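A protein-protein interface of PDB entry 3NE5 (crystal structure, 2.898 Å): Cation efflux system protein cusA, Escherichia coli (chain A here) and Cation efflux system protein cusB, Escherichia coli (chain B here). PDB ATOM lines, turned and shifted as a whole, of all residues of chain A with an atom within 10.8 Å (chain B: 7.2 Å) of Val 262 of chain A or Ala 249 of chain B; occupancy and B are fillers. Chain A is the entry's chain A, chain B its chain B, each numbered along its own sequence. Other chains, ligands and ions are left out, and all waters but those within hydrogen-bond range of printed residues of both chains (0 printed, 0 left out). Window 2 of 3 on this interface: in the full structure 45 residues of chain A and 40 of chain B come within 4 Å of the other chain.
ND2 of Asn 113 of chain B sits at hydrogen-bond distance from O of Asn 260 of chain A (2.9 Å).
The backbone carbonyl oxygen (O) of Pro 111 of chain B is in hydrogen-bond range of the backbone NH (N) of Ala 249 of chain B. N of Glu 252 of chain B lies within hydrogen-bond range of O of Arg 292 of chain B. OD2 of Asp 288 of chain B is in hydrogen-bond range of OG1 of Thr 291 of chain B (2.9 Å). The side-chain hydroxyl of Thr 293 of chain B is in hydrogen-bond range of the side-chain amide nitrogen of Gln 295 of chain B, at 2.9 Å. The backbone carbonyl oxygen (O) of Val 264 of chain A lies within hydrogen-bond range of the backbone NH (N) of Leu 255 of chain A (2.9 Å). The guanidinium group (NH2) of Arg 267 of chain A lies within salt-bridge range of the side-chain carboxylate (OD1) of Asp 268 of chain A.
Among the printed residues, merely in contact across the chains: Tyr 206 of chain A with Arg 292 of chain B (3.5 Å), Gly 261 of chain A with Pro 111 of chain B (3.97 Å), Val 262 of chain A with Ala 249 of chain B (3.5 Å), Val 262 of chain A with Thr 291 of chain B (3.5 Å), Val 262 of chain A with Thr 293 of chain B (3.9 Å), Val 264 of chain A with Thr 291 of chain B (3.98 Å) and Arg 267 of chain A with Pro 251 of chain B (3.5 Å).
Of the printed residues of chain B, Tyr 206 of chain A touches Arg 292 (3.5 Å). Printed residues of chain B within 4 Å of Gly 261 of chain A: Pro 111 (3.97 Å). Val 262 of chain A touches just these residues of chain B: Ala 249, Thr 291 and Thr 293. Of the printed residues of chain B, Val 264 of chain A touches Thr 291. Tyr 265 of chain A touches none of the printed residues of chain B. Of the printed residues of chain B, Arg 267 of chain A touches Pro 251 (3.5 Å). No residue of chain A comes within 4 Å of Phe 110 of chain B. Of the printed residues of chain A, Asn 113 of chain B touches Asn 260. Of chain A, only Val 262 (3.5 Å) comes within 4 Å of Ala 249 of chain B. Ile 250 of chain B touches none of the printed residues of chain A. Of the printed residues of chain A, Pro 251 of chain B touches Arg 267. Thr 291 of chain B touches just these residues of chain A: Val 262 (3.5 Å) and Val 264 (3.98 Å). Of the printed residues of chain A, Thr 293 of chain B touches Val 262. Leu 315 of chain B touches none of the printed residues of chain A. The nearest residue of chain A that does not touch Ala 249 of chain B is Pro 263 of chain A (6.8 Å).
Of the 20 printed residues of chain B, 7 touch a printed residue of chain A. Hydrophobic or aromatic side chains of chain B that line the printed part of chain A: Pro 111, Ala 249 and Pro 251.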
ATOM      1  N   TYR A 206      10.755   7.074 -10.532  1.00  0.00           N
ATOM      2  CA  TYR A 206      11.644   6.559  -9.499  1.00  0.00           C
ATOM      3  C   TYR A 206      11.087   6.792  -8.101  1.00  0.00           C
ATOM      4  O   TYR A 206      11.690   6.391  -7.107  1.00  0.00           O
ATOM      5  CB  TYR A 206      13.037   7.175  -9.634  1.00  0.00           C
ATOM      6  CG  TYR A 206      13.813   6.648 -10.819  1.00  0.00           C
ATOM      7  CD1 TYR A 206      14.739   5.621 -10.669  1.00  0.00           C
ATOM      8  CD2 TYR A 206      13.614   7.170 -12.091  1.00  0.00           C
ATOM      9  CE1 TYR A 206      15.445   5.135 -11.752  1.00  0.00           C
ATOM     10  CE2 TYR A 206      14.318   6.690 -13.178  1.00  0.00           C
ATOM     11  CZ  TYR A 206      15.231   5.673 -13.003  1.00  0.00           C
ATOM     12  OH  TYR A 206      15.932   5.194 -14.084  1.00  0.00           O
ATOM     13  N   ILE A 208      10.653   9.648  -6.342  1.00  0.00           N
ATOM     14  CA  ILE A 208      11.497  10.532  -5.551  1.00  0.00           C
ATOM     15  C   ILE A 208      11.026  11.974  -5.682  1.00  0.00           C
ATOM     16  O   ILE A 208      10.895  12.495  -6.787  1.00  0.00           O
ATOM     17  CB  ILE A 208      12.969  10.430  -5.974  1.00  0.00           C
ATOM     18  CG1 ILE A 208      13.473   8.999  -5.779  1.00  0.00           C
ATOM     19  CG2 ILE A 208      13.819  11.403  -5.178  1.00  0.00           C
ATOM     20  CD1 ILE A 208      14.948   8.834  -6.043  1.00  0.00           C
ATOM     21  N   ILE A 253      25.146  11.357  -6.349  1.00  0.00           N
ATOM     22  CA  ILE A 253      24.433  11.750  -5.142  1.00  0.00           C
ATOM     23  C   ILE A 253      23.382  10.681  -4.891  1.00  0.00           C
ATOM     24  O   ILE A 253      22.530  10.435  -5.744  1.00  0.00           O
ATOM     25  CB  ILE A 253      23.707  13.097  -5.323  1.00  0.00           C
ATOM     26  CG1 ILE A 253      24.694  14.215  -5.674  1.00  0.00           C
ATOM     27  CG2 ILE A 253      22.907  13.442  -4.072  1.00  0.00           C
ATOM     28  CD1 ILE A 253      25.192  15.004  -4.493  1.00  0.00           C
ATOM     29  N   VAL A 254      23.437  10.040  -3.730  1.00  0.00           N
ATOM     30  CA  VAL A 254      22.500   8.964  -3.432  1.00  0.00           C
ATOM     31  C   VAL A 254      21.140   9.506  -3.001  1.00  0.00           C
ATOM     32  O   VAL A 254      21.056  10.457  -2.224  1.00  0.00           O
ATOM     33  CB  VAL A 254      23.050   8.002  -2.359  1.00  0.00           C
ATOM     34  CG1 VAL A 254      23.207   8.715  -1.021  1.00  0.00           C
ATOM     35  CG2 VAL A 254      22.144   6.790  -2.228  1.00  0.00           C
ATOM     36  N   LEU A 255      20.076   8.899  -3.514  1.00  0.00           N
ATOM     37  CA  LEU A 255      18.722   9.352  -3.218  1.00  0.00           C
ATOM     38  C   LEU A 255      17.916   8.290  -2.480  1.00  0.00           C
ATOM     39  O   LEU A 255      17.008   8.610  -1.713  1.00  0.00           O
ATOM     40  CB  LEU A 255      17.994   9.736  -4.509  1.00  0.00           C
ATOM     41  CG  LEU A 255      18.639  10.796  -5.405  1.00  0.00           C
ATOM     42  CD1 LEU A 255      17.887  10.914  -6.725  1.00  0.00           C
ATOM     43  CD2 LEU A 255      18.696  12.140  -4.696  1.00  0.00           C
ATOM     44  N   LYS A 256      18.262   7.027  -2.710  1.00  0.00           N
ATOM     45  CA  LYS A 256      17.448   5.910  -2.251  1.00  0.00           C
ATOM     46  C   LYS A 256      18.243   4.614  -2.384  1.00  0.00           C
ATOM     47  O   LYS A 256      19.087   4.489  -3.272  1.00  0.00           O
ATOM     48  CB  LYS A 256      16.182   5.834  -3.107  1.00  0.00           C
ATOM     49  CG  LYS A 256      15.040   5.032  -2.522  1.00  0.00           C
ATOM     50  CD  LYS A 256      13.876   4.988  -3.503  1.00  0.00           C
ATOM     51  CE  LYS A 256      12.585   4.549  -2.832  1.00  0.00           C
ATOM     52  NZ  LYS A 256      11.411   4.735  -3.732  1.00  0.00           N
ATOM     53  N   ALA A 257      17.978   3.649  -1.509  1.00  0.00           N
ATOM     54  CA  ALA A 257      18.694   2.376  -1.557  1.00  0.00           C
ATOM     55  C   ALA A 257      17.835   1.190  -1.127  1.00  0.00           C
ATOM     56  O   ALA A 257      17.229   1.202  -0.056  1.00  0.00           O
ATOM     57  CB  ALA A 257      19.962   2.448  -0.718  1.00  0.00           C
ATOM     58  N   SER A 258      17.797   0.165  -1.971  1.00  0.00           N
ATOM     59  CA  SER A 258      17.053  -1.055  -1.676  1.00  0.00           C
ATOM     60  C   SER A 258      17.812  -1.923  -0.678  1.00  0.00           C
ATOM     61  O   SER A 258      18.996  -1.703  -0.427  1.00  0.00           O
ATOM     62  CB  SER A 258      16.808  -1.845  -2.964  1.00  0.00           C
ATOM     63  OG  SER A 258      18.033  -2.296  -3.521  1.00  0.00           O
ATOM     64  N   GLU A 259      17.127  -2.910  -0.110  1.00  0.00           N
ATOM     65  CA  GLU A 259      17.770  -3.875   0.773  1.00  0.00           C
ATOM     66  C   GLU A 259      18.866  -4.600   0.002  1.00  0.00           C
ATOM     67  O   GLU A 259      19.905  -4.961   0.561  1.00  0.00           O
ATOM     68  CB  GLU A 259      16.748  -4.883   1.298  1.00  0.00           C
ATOM     69  CG  GLU A 259      15.522  -4.252   1.936  1.00  0.00           C
ATOM     70  CD  GLU A 259      14.416  -5.259   2.196  1.00  0.00           C
ATOM     71  OE1 GLU A 259      13.527  -4.968   3.023  1.00  0.00           O
ATOM     72  OE2 GLU A 259      14.435  -6.342   1.572  1.00  0.00           O
ATOM     73  N   ASN A 260      18.614  -4.807  -1.287  1.00  0.00           N
ATOM     74  CA  ASN A 260      19.572  -5.435  -2.191  1.00  0.00           C
ATOM     75  C   ASN A 260      20.903  -4.703  -2.229  1.00  0.00           C
ATOM     76  O   ASN A 260      21.949  -5.308  -2.452  1.00  0.00           O
ATOM     77  CB  ASN A 260      18.994  -5.503  -3.605  1.00  0.00           C
ATOM     78  CG  ASN A 260      18.487  -6.883  -3.963  1.00  0.00           C
ATOM     79  OD1 ASN A 260      18.940  -7.886  -3.411  1.00  0.00           O
ATOM     80  ND2 ASN A 260      17.551  -6.943  -4.902  1.00  0.00           N
ATOM     81  N   GLY A 261      20.856  -3.395  -2.016  1.00  0.00           N
ATOM     82  CA  GLY A 261      22.051  -2.580  -2.086  1.00  0.00           C
ATOM     83  C   GLY A 261      22.138  -1.876  -3.422  1.00  0.00           C
ATOM     84  O   GLY A 261      23.175  -1.323  -3.772  1.00  0.00           O
ATOM     85  N   VAL A 262      21.043  -1.909  -4.174  1.00  0.00           N
ATOM     86  CA  VAL A 262      20.965  -1.181  -5.432  1.00  0.00           C
ATOM     87  C   VAL A 262      20.472   0.231  -5.160  1.00  0.00           C
ATOM     88  O   VAL A 262      19.334   0.425  -4.734  1.00  0.00           O
ATOM     89  CB  VAL A 262      20.024  -1.867  -6.435  1.00  0.00           C
ATOM     90  CG1 VAL A 262      19.923  -1.045  -7.710  1.00  0.00           C
ATOM     91  CG2 VAL A 262      20.508  -3.277  -6.736  1.00  0.00           C
ATOM     92  N   PRO A 263      21.339   1.226  -5.388  1.00  0.00           N
ATOM     93  CA  PRO A 263      21.024   2.620  -5.078  1.00  0.00           C
ATOM     94  C   PRO A 263      20.413   3.343  -6.270  1.00  0.00           C
ATOM     95  O   PRO A 263      20.630   2.941  -7.413  1.00  0.00           O
ATOM     96  CB  PRO A 263      22.403   3.227  -4.766  1.00  0.00           C
ATOM     97  CG  PRO A 263      23.417   2.094  -4.948  1.00  0.00           C
ATOM     98  CD  PRO A 263      22.740   1.074  -5.797  1.00  0.00           C
ATOM     99  N   VAL A 264      19.651   4.396  -5.998  1.00  0.00           N
ATOM    100  CA  VAL A 264      19.170   5.288  -7.044  1.00  0.00           C
ATOM    101  C   VAL A 264      19.894   6.621  -6.917  1.00  0.00           C
ATOM    102  O   VAL A 264      19.833   7.273  -5.874  1.00  0.00           O
ATOM    103  CB  VAL A 264      17.654   5.525  -6.951  1.00  0.00           C
ATOM    104  CG1 VAL A 264      17.220   6.576  -7.963  1.00  0.00           C
ATOM    105  CG2 VAL A 264      16.903   4.226  -7.168  1.00  0.00           C
ATOM    106  N   TYR A 265      20.583   7.017  -7.979  1.00  0.00           N
ATOM    107  CA  TYR A 265      21.419   8.210  -7.947  1.00  0.00           C
ATOM    108  C   TYR A 265      20.737   9.442  -8.543  1.00  0.00           C
ATOM    109  O   TYR A 265      19.678   9.348  -9.162  1.00  0.00           O
ATOM    110  CB  TYR A 265      22.733   7.949  -8.681  1.00  0.00           C
ATOM    111  CG  TYR A 265      23.666   6.992  -7.974  1.00  0.00           C
ATOM    112  CD1 TYR A 265      23.877   5.709  -8.460  1.00  0.00           C
ATOM    113  CD2 TYR A 265      24.346   7.377  -6.826  1.00  0.00           C
ATOM    114  CE1 TYR A 265      24.736   4.835  -7.821  1.00  0.00           C
ATOM    115  CE2 TYR A 265      25.208   6.511  -6.181  1.00  0.00           C
ATOM    116  CZ  TYR A 265      25.397   5.242  -6.682  1.00  0.00           C
ATOM    117  OH  TYR A 265      26.252   4.374  -6.041  1.00  0.00           O
ATOM    118  N   ARG A 267      21.765  11.002 -10.972  1.00  0.00           N
ATOM    119  CA  ARG A 267      21.863  10.855 -12.422  1.00  0.00           C
ATOM    120  C   ARG A 267      20.641  10.139 -12.981  1.00  0.00           C
ATOM    121  O   ARG A 267      20.404  10.143 -14.188  1.00  0.00           O
ATOM    122  CB  ARG A 267      23.126  10.083 -12.817  1.00  0.00           C
ATOM    123  CG  ARG A 267      23.180   8.653 -12.292  1.00  0.00           C
ATOM    124  CD  ARG A 267      23.860   7.712 -13.282  1.00  0.00           C
ATOM    125  NE  ARG A 267      24.295   6.467 -12.653  1.00  0.00           N
ATOM    126  CZ  ARG A 267      23.473   5.503 -12.248  1.00  0.00           C
ATOM    127  NH1 ARG A 267      23.958   4.405 -11.686  1.00  0.00           N
ATOM    128  NH2 ARG A 267      22.164   5.637 -12.398  1.00  0.00           N
ATOM    129  N   ASP A 268      19.869   9.520 -12.095  1.00  0.00           N
ATOM    130  CA  ASP A 268      18.700   8.755 -12.508  1.00  0.00           C
ATOM    131  C   ASP A 268      17.494   9.642 -12.764  1.00  0.00           C
ATOM    132  O   ASP A 268      16.629   9.306 -13.571  1.00  0.00           O
ATOM    133  CB  ASP A 268      18.356   7.702 -11.456  1.00  0.00           C
ATOM    134  CG  ASP A 268      19.316   6.535 -11.473  1.00  0.00           C
ATOM    135  OD1 ASP A 268      19.613   6.036 -12.578  1.00  0.00           O
ATOM    136  OD2 ASP A 268      19.767   6.115 -10.387  1.00  0.00           O
ATOM    137  N   SER B 109      30.900   0.700 -12.617  1.00  0.00           N
ATOM    138  CA  SER B 109      30.895  -0.381 -11.641  1.00  0.00           C
ATOM    139  C   SER B 109      29.476  -0.598 -11.129  1.00  0.00           C
ATOM    140  O   SER B 109      28.924   0.240 -10.410  1.00  0.00           O
ATOM    141  CB  SER B 109      31.837  -0.060 -10.481  1.00  0.00           C
ATOM    142  OG  SER B 109      33.077   0.426 -10.961  1.00  0.00           O
ATOM    143  N   PHE B 110      28.888  -1.723 -11.510  1.00  0.00           N
ATOM    144  CA  PHE B 110      27.516  -2.019 -11.151  1.00  0.00           C
ATOM    145  C   PHE B 110      27.434  -2.792  -9.825  1.00  0.00           C
ATOM    146  O   PHE B 110      28.238  -3.692  -9.588  1.00  0.00           O
ATOM    147  CB  PHE B 110      26.854  -2.818 -12.278  1.00  0.00           C
ATOM    148  CG  PHE B 110      27.096  -2.265 -13.668  1.00  0.00           C
ATOM    149  CD1 PHE B 110      26.563  -1.039 -14.055  1.00  0.00           C
ATOM    150  CD2 PHE B 110      27.821  -3.000 -14.603  1.00  0.00           C
ATOM    151  CE1 PHE B 110      26.769  -0.544 -15.338  1.00  0.00           C
ATOM    152  CE2 PHE B 110      28.027  -2.512 -15.885  1.00  0.00           C
ATOM    153  CZ  PHE B 110      27.503  -1.284 -16.252  1.00  0.00           C
ATOM    154  N   PRO B 111      26.472  -2.425  -8.952  1.00  0.00           N
ATOM    155  CA  PRO B 111      26.184  -3.126  -7.697  1.00  0.00           C
ATOM    156  C   PRO B 111      25.741  -4.541  -8.013  1.00  0.00           C
ATOM    157  O   PRO B 111      24.993  -4.744  -8.973  1.00  0.00           O
ATOM    158  CB  PRO B 111      24.986  -2.348  -7.148  1.00  0.00           C
ATOM    159  CG  PRO B 111      24.356  -1.749  -8.368  1.00  0.00           C
ATOM    160  CD  PRO B 111      25.568  -1.278  -9.113  1.00  0.00           C
ATOM    161  N   ALA B 112      26.173  -5.504  -7.207  1.00  0.00           N
ATOM    162  CA  ALA B 112      25.882  -6.912  -7.463  1.00  0.00           C
ATOM    163  C   ALA B 112      25.784  -7.701  -6.161  1.00  0.00           C
ATOM    164  O   ALA B 112      26.354  -7.317  -5.141  1.00  0.00           O
ATOM    165  CB  ALA B 112      26.946  -7.508  -8.355  1.00  0.00           C
ATOM    166  N   ASN B 113      25.063  -8.814  -6.202  1.00  0.00           N
ATOM    167  CA  ASN B 113      24.900  -9.654  -5.024  1.00  0.00           C
ATOM    168  C   ASN B 113      25.171 -11.121  -5.306  1.00  0.00           C
ATOM    169  O   ASN B 113      24.882 -11.617  -6.392  1.00  0.00           O
ATOM    170  CB  ASN B 113      23.488  -9.517  -4.459  1.00  0.00           C
ATOM    171  CG  ASN B 113      23.240  -8.171  -3.826  1.00  0.00           C
ATOM    172  OD1 ASN B 113      23.789  -7.855  -2.772  1.00  0.00           O
ATOM    173  ND2 ASN B 113      22.394  -7.370  -4.462  1.00  0.00           N
ATOM    174  N   THR B 247      24.242 -11.760  -9.293  1.00  0.00           N
ATOM    175  CA  THR B 247      23.376 -10.927 -10.117  1.00  0.00           C
ATOM    176  C   THR B 247      23.757  -9.458  -9.983  1.00  0.00           C
ATOM    177  O   THR B 247      23.927  -8.949  -8.876  1.00  0.00           O
ATOM    178  CB  THR B 247      21.898 -11.094  -9.729  1.00  0.00           C
ATOM    179  OG1 THR B 247      21.606 -12.483  -9.530  1.00  0.00           O
ATOM    180  CG2 THR B 247      20.999 -10.538 -10.820  1.00  0.00           C
ATOM    181  N   ALA B 248      23.893  -8.779 -11.116  1.00  0.00           N
ATOM    182  CA  ALA B 248      24.251  -7.367 -11.119  1.00  0.00           C
ATOM    183  C   ALA B 248      23.082  -6.514 -11.593  1.00  0.00           C
ATOM    184  O   ALA B 248      22.348  -6.901 -12.502  1.00  0.00           O
ATOM    185  CB  ALA B 248      25.467  -7.132 -12.000  1.00  0.00           C
ATOM    186  N   ALA B 249      22.913  -5.354 -10.969  1.00  0.00           N
ATOM    187  CA  ALA B 249      21.878  -4.412 -11.378  1.00  0.00           C
ATOM    188  C   ALA B 249      22.486  -3.295 -12.219  1.00  0.00           C
ATOM    189  O   ALA B 249      23.294  -2.504 -11.732  1.00  0.00           O
ATOM    190  CB  ALA B 249      21.161  -3.842 -10.164  1.00  0.00           C
ATOM    191  N   ILE B 250      22.092  -3.239 -13.487  1.00  0.00           N
ATOM    192  CA  ILE B 250      22.642  -2.264 -14.421  1.00  0.00           C
ATOM    193  C   ILE B 250      21.600  -1.223 -14.815  1.00  0.00           C
ATOM    194  O   ILE B 250      20.489  -1.576 -15.206  1.00  0.00           O
ATOM    195  CB  ILE B 250      23.169  -2.960 -15.687  1.00  0.00           C
ATOM    196  CG1 ILE B 250      24.298  -3.927 -15.324  1.00  0.00           C
ATOM    197  CG2 ILE B 250      23.645  -1.936 -16.704  1.00  0.00           C
ATOM    198  CD1 ILE B 250      24.732  -4.817 -16.468  1.00  0.00           C
ATOM    199  N   PRO B 251      21.958   0.066 -14.714  1.00  0.00           N
ATOM    200  CA  PRO B 251      21.033   1.148 -15.069  1.00  0.00           C
ATOM    201  C   PRO B 251      20.454   0.955 -16.462  1.00  0.00           C
ATOM    202  O   PRO B 251      21.196   0.911 -17.442  1.00  0.00           O
ATOM    203  CB  PRO B 251      21.920   2.395 -15.038  1.00  0.00           C
ATOM    204  CG  PRO B 251      23.012   2.054 -14.092  1.00  0.00           C
ATOM    205  CD  PRO B 251      23.262   0.579 -14.258  1.00  0.00           C
ATOM    206  N   GLU B 252      19.135   0.834 -16.534  1.00  0.00           N
ATOM    207  CA  GLU B 252      18.423   0.645 -17.792  1.00  0.00           C
ATOM    208  C   GLU B 252      18.938   1.519 -18.938  1.00  0.00           C
ATOM    209  O   GLU B 252      18.935   1.100 -20.094  1.00  0.00           O
ATOM    210  CB  GLU B 252      16.930   0.892 -17.571  1.00  0.00           C
ATOM    211  CG  GLU B 252      16.294   1.801 -18.599  1.00  0.00           C
ATOM    212  CD  GLU B 252      15.056   2.489 -18.075  1.00  0.00           C
ATOM    213  OE1 GLU B 252      15.087   3.726 -17.907  1.00  0.00           O
ATOM    214  OE2 GLU B 252      14.056   1.793 -17.815  1.00  0.00           O
ATOM    215  N   ASP B 288      14.043  -4.593 -12.847  1.00  0.00           N
ATOM    216  CA  ASP B 288      13.459  -4.199 -11.574  1.00  0.00           C
ATOM    217  C   ASP B 288      12.781  -2.848 -11.732  1.00  0.00           C
ATOM    218  O   ASP B 288      13.287  -1.969 -12.429  1.00  0.00           O
ATOM    219  CB  ASP B 288      14.538  -4.132 -10.491  1.00  0.00           C
ATOM    220  CG  ASP B 288      13.972  -3.823  -9.121  1.00  0.00           C
ATOM    221  OD1 ASP B 288      12.840  -4.263  -8.828  1.00  0.00           O
ATOM    222  OD2 ASP B 288      14.663  -3.147  -8.330  1.00  0.00           O
ATOM    223  N   THR B 291      14.015   0.083  -8.557  1.00  0.00           N
ATOM    224  CA  THR B 291      15.174   0.683  -9.191  1.00  0.00           C
ATOM    225  C   THR B 291      15.118   0.226 -10.636  1.00  0.00           C
ATOM    226  O   THR B 291      15.106  -0.971 -10.908  1.00  0.00           O
ATOM    227  CB  THR B 291      16.477   0.187  -8.566  1.00  0.00           C
ATOM    228  OG1 THR B 291      16.705  -1.176  -8.947  1.00  0.00           O
ATOM    229  CG2 THR B 291      16.406   0.279  -7.052  1.00  0.00           C
ATOM    230  N   ARG B 292      15.055   1.166 -11.568  1.00  0.00           N
ATOM    231  CA  ARG B 292      14.941   0.797 -12.971  1.00  0.00           C
ATOM    232  C   ARG B 292      16.266   0.238 -13.458  1.00  0.00           C
ATOM    233  O   ARG B 292      17.069   0.953 -14.049  1.00  0.00           O
ATOM    234  CB  ARG B 292      14.537   2.008 -13.802  1.00  0.00           C
ATOM    235  CG  ARG B 292      13.336   2.745 -13.246  1.00  0.00           C
ATOM    236  CD  ARG B 292      12.066   1.973 -13.515  1.00  0.00           C
ATOM    237  NE  ARG B 292      10.891   2.651 -12.978  1.00  0.00           N
ATOM    238  CZ  ARG B 292       9.645   2.380 -13.347  1.00  0.00           C
ATOM    239  NH1 ARG B 292       9.410   1.451 -14.262  1.00  0.00           N
ATOM    240  NH2 ARG B 292       8.633   3.043 -12.810  1.00  0.00           N
ATOM    241  N   THR B 293      16.491  -1.045 -13.202  1.00  0.00           N
ATOM    242  CA  THR B 293      17.775  -1.661 -13.502  1.00  0.00           C
ATOM    243  C   THR B 293      17.611  -2.986 -14.226  1.00  0.00           C
ATOM    244  O   THR B 293      16.748  -3.793 -13.882  1.00  0.00           O
ATOM    245  CB  THR B 293      18.577  -1.930 -12.216  1.00  0.00           C
ATOM    246  OG1 THR B 293      17.864  -2.868 -11.399  1.00  0.00           O
ATOM    247  CG2 THR B 293      18.790  -0.643 -11.436  1.00  0.00           C
ATOM    248  N   LEU B 294      18.452  -3.203 -15.229  1.00  0.00           N
ATOM    249  CA  LEU B 294      18.536  -4.492 -15.892  1.00  0.00           C
ATOM    250  C   LEU B 294      19.093  -5.497 -14.895  1.00  0.00           C
ATOM    251  O   LEU B 294      19.791  -5.122 -13.953  1.00  0.00           O
ATOM    252  CB  LEU B 294      19.461  -4.399 -17.104  1.00  0.00           C
ATOM    253  CG  LEU B 294      19.085  -3.376 -18.172  1.00  0.00           C
ATOM    254  CD1 LEU B 294      20.291  -3.058 -19.033  1.00  0.00           C
ATOM    255  CD2 LEU B 294      17.942  -3.897 -19.022  1.00  0.00           C
ATOM    256  N   GLN B 295      18.785  -6.774 -15.095  1.00  0.00           N
ATOM    257  CA  GLN B 295      19.295  -7.820 -14.215  1.00  0.00           C
ATOM    258  C   GLN B 295      20.181  -8.796 -14.979  1.00  0.00           C
ATOM    259  O   GLN B 295      19.713  -9.540 -15.838  1.00  0.00           O
ATOM    260  CB  GLN B 295      18.148  -8.564 -13.527  1.00  0.00           C
ATOM    261  CG  GLN B 295      17.243  -7.677 -12.685  1.00  0.00           C
ATOM    262  CD  GLN B 295      17.968  -7.031 -11.517  1.00  0.00           C
ATOM    263  OE1 GLN B 295      18.724  -7.687 -10.800  1.00  0.00           O
ATOM    264  NE2 GLN B 295      17.733  -5.739 -11.317  1.00  0.00           N
ATOM    265  N   LEU B 296      21.467  -8.781 -14.659  1.00  0.00           N
ATOM    266  CA  LEU B 296      22.431  -9.646 -15.322  1.00  0.00           C
ATOM    267  C   LEU B 296      22.898 -10.728 -14.356  1.00  0.00           C
ATOM    268  O   LEU B 296      23.448 -10.429 -13.297  1.00  0.00           O
ATOM    269  CB  LEU B 296      23.615  -8.819 -15.828  1.00  0.00           C
ATOM    270  CG  LEU B 296      24.648  -9.498 -16.725  1.00  0.00           C
ATOM    271  CD1 LEU B 296      25.459  -8.453 -17.474  1.00  0.00           C
ATOM    272  CD2 LEU B 296      25.555 -10.403 -15.913  1.00  0.00           C
ATOM    273  N   ASN B 312      28.203  -9.066  -0.771  1.00  0.00           N
ATOM    274  CA  ASN B 312      28.165  -8.013  -1.773  1.00  0.00           C
ATOM    275  C   ASN B 312      29.242  -8.235  -2.819  1.00  0.00           C
ATOM    276  O   ASN B 312      30.287  -8.817  -2.535  1.00  0.00           O
ATOM    277  CB  ASN B 312      28.365  -6.647  -1.121  1.00  0.00           C
ATOM    278  CG  ASN B 312      27.063  -5.997  -0.724  1.00  0.00           C
ATOM    279  OD1 ASN B 312      26.086  -6.036  -1.470  1.00  0.00           O
ATOM    280  ND2 ASN B 312      27.042  -5.385   0.452  1.00  0.00           N
ATOM    281  N   LEU B 315      30.274  -5.586 -10.296  1.00  0.00           N
ATOM    282  CA  LEU B 315      30.500  -5.996 -11.676  1.00  0.00           C
ATOM    283  C   LEU B 315      30.986  -4.813 -12.506  1.00  0.00           C
ATOM    284  O   LEU B 315      30.239  -3.866 -12.755  1.00  0.00           O
ATOM    285  CB  LEU B 315      29.232  -6.593 -12.289  1.00  0.00           C
ATOM    286  CG  LEU B 315      29.451  -7.373 -13.588  1.00  0.00           C
ATOM    287  CD1 LEU B 315      30.321  -8.589 -13.329  1.00  0.00           C
ATOM    288  CD2 LEU B 315      28.127  -7.786 -14.205  1.00  0.00           C
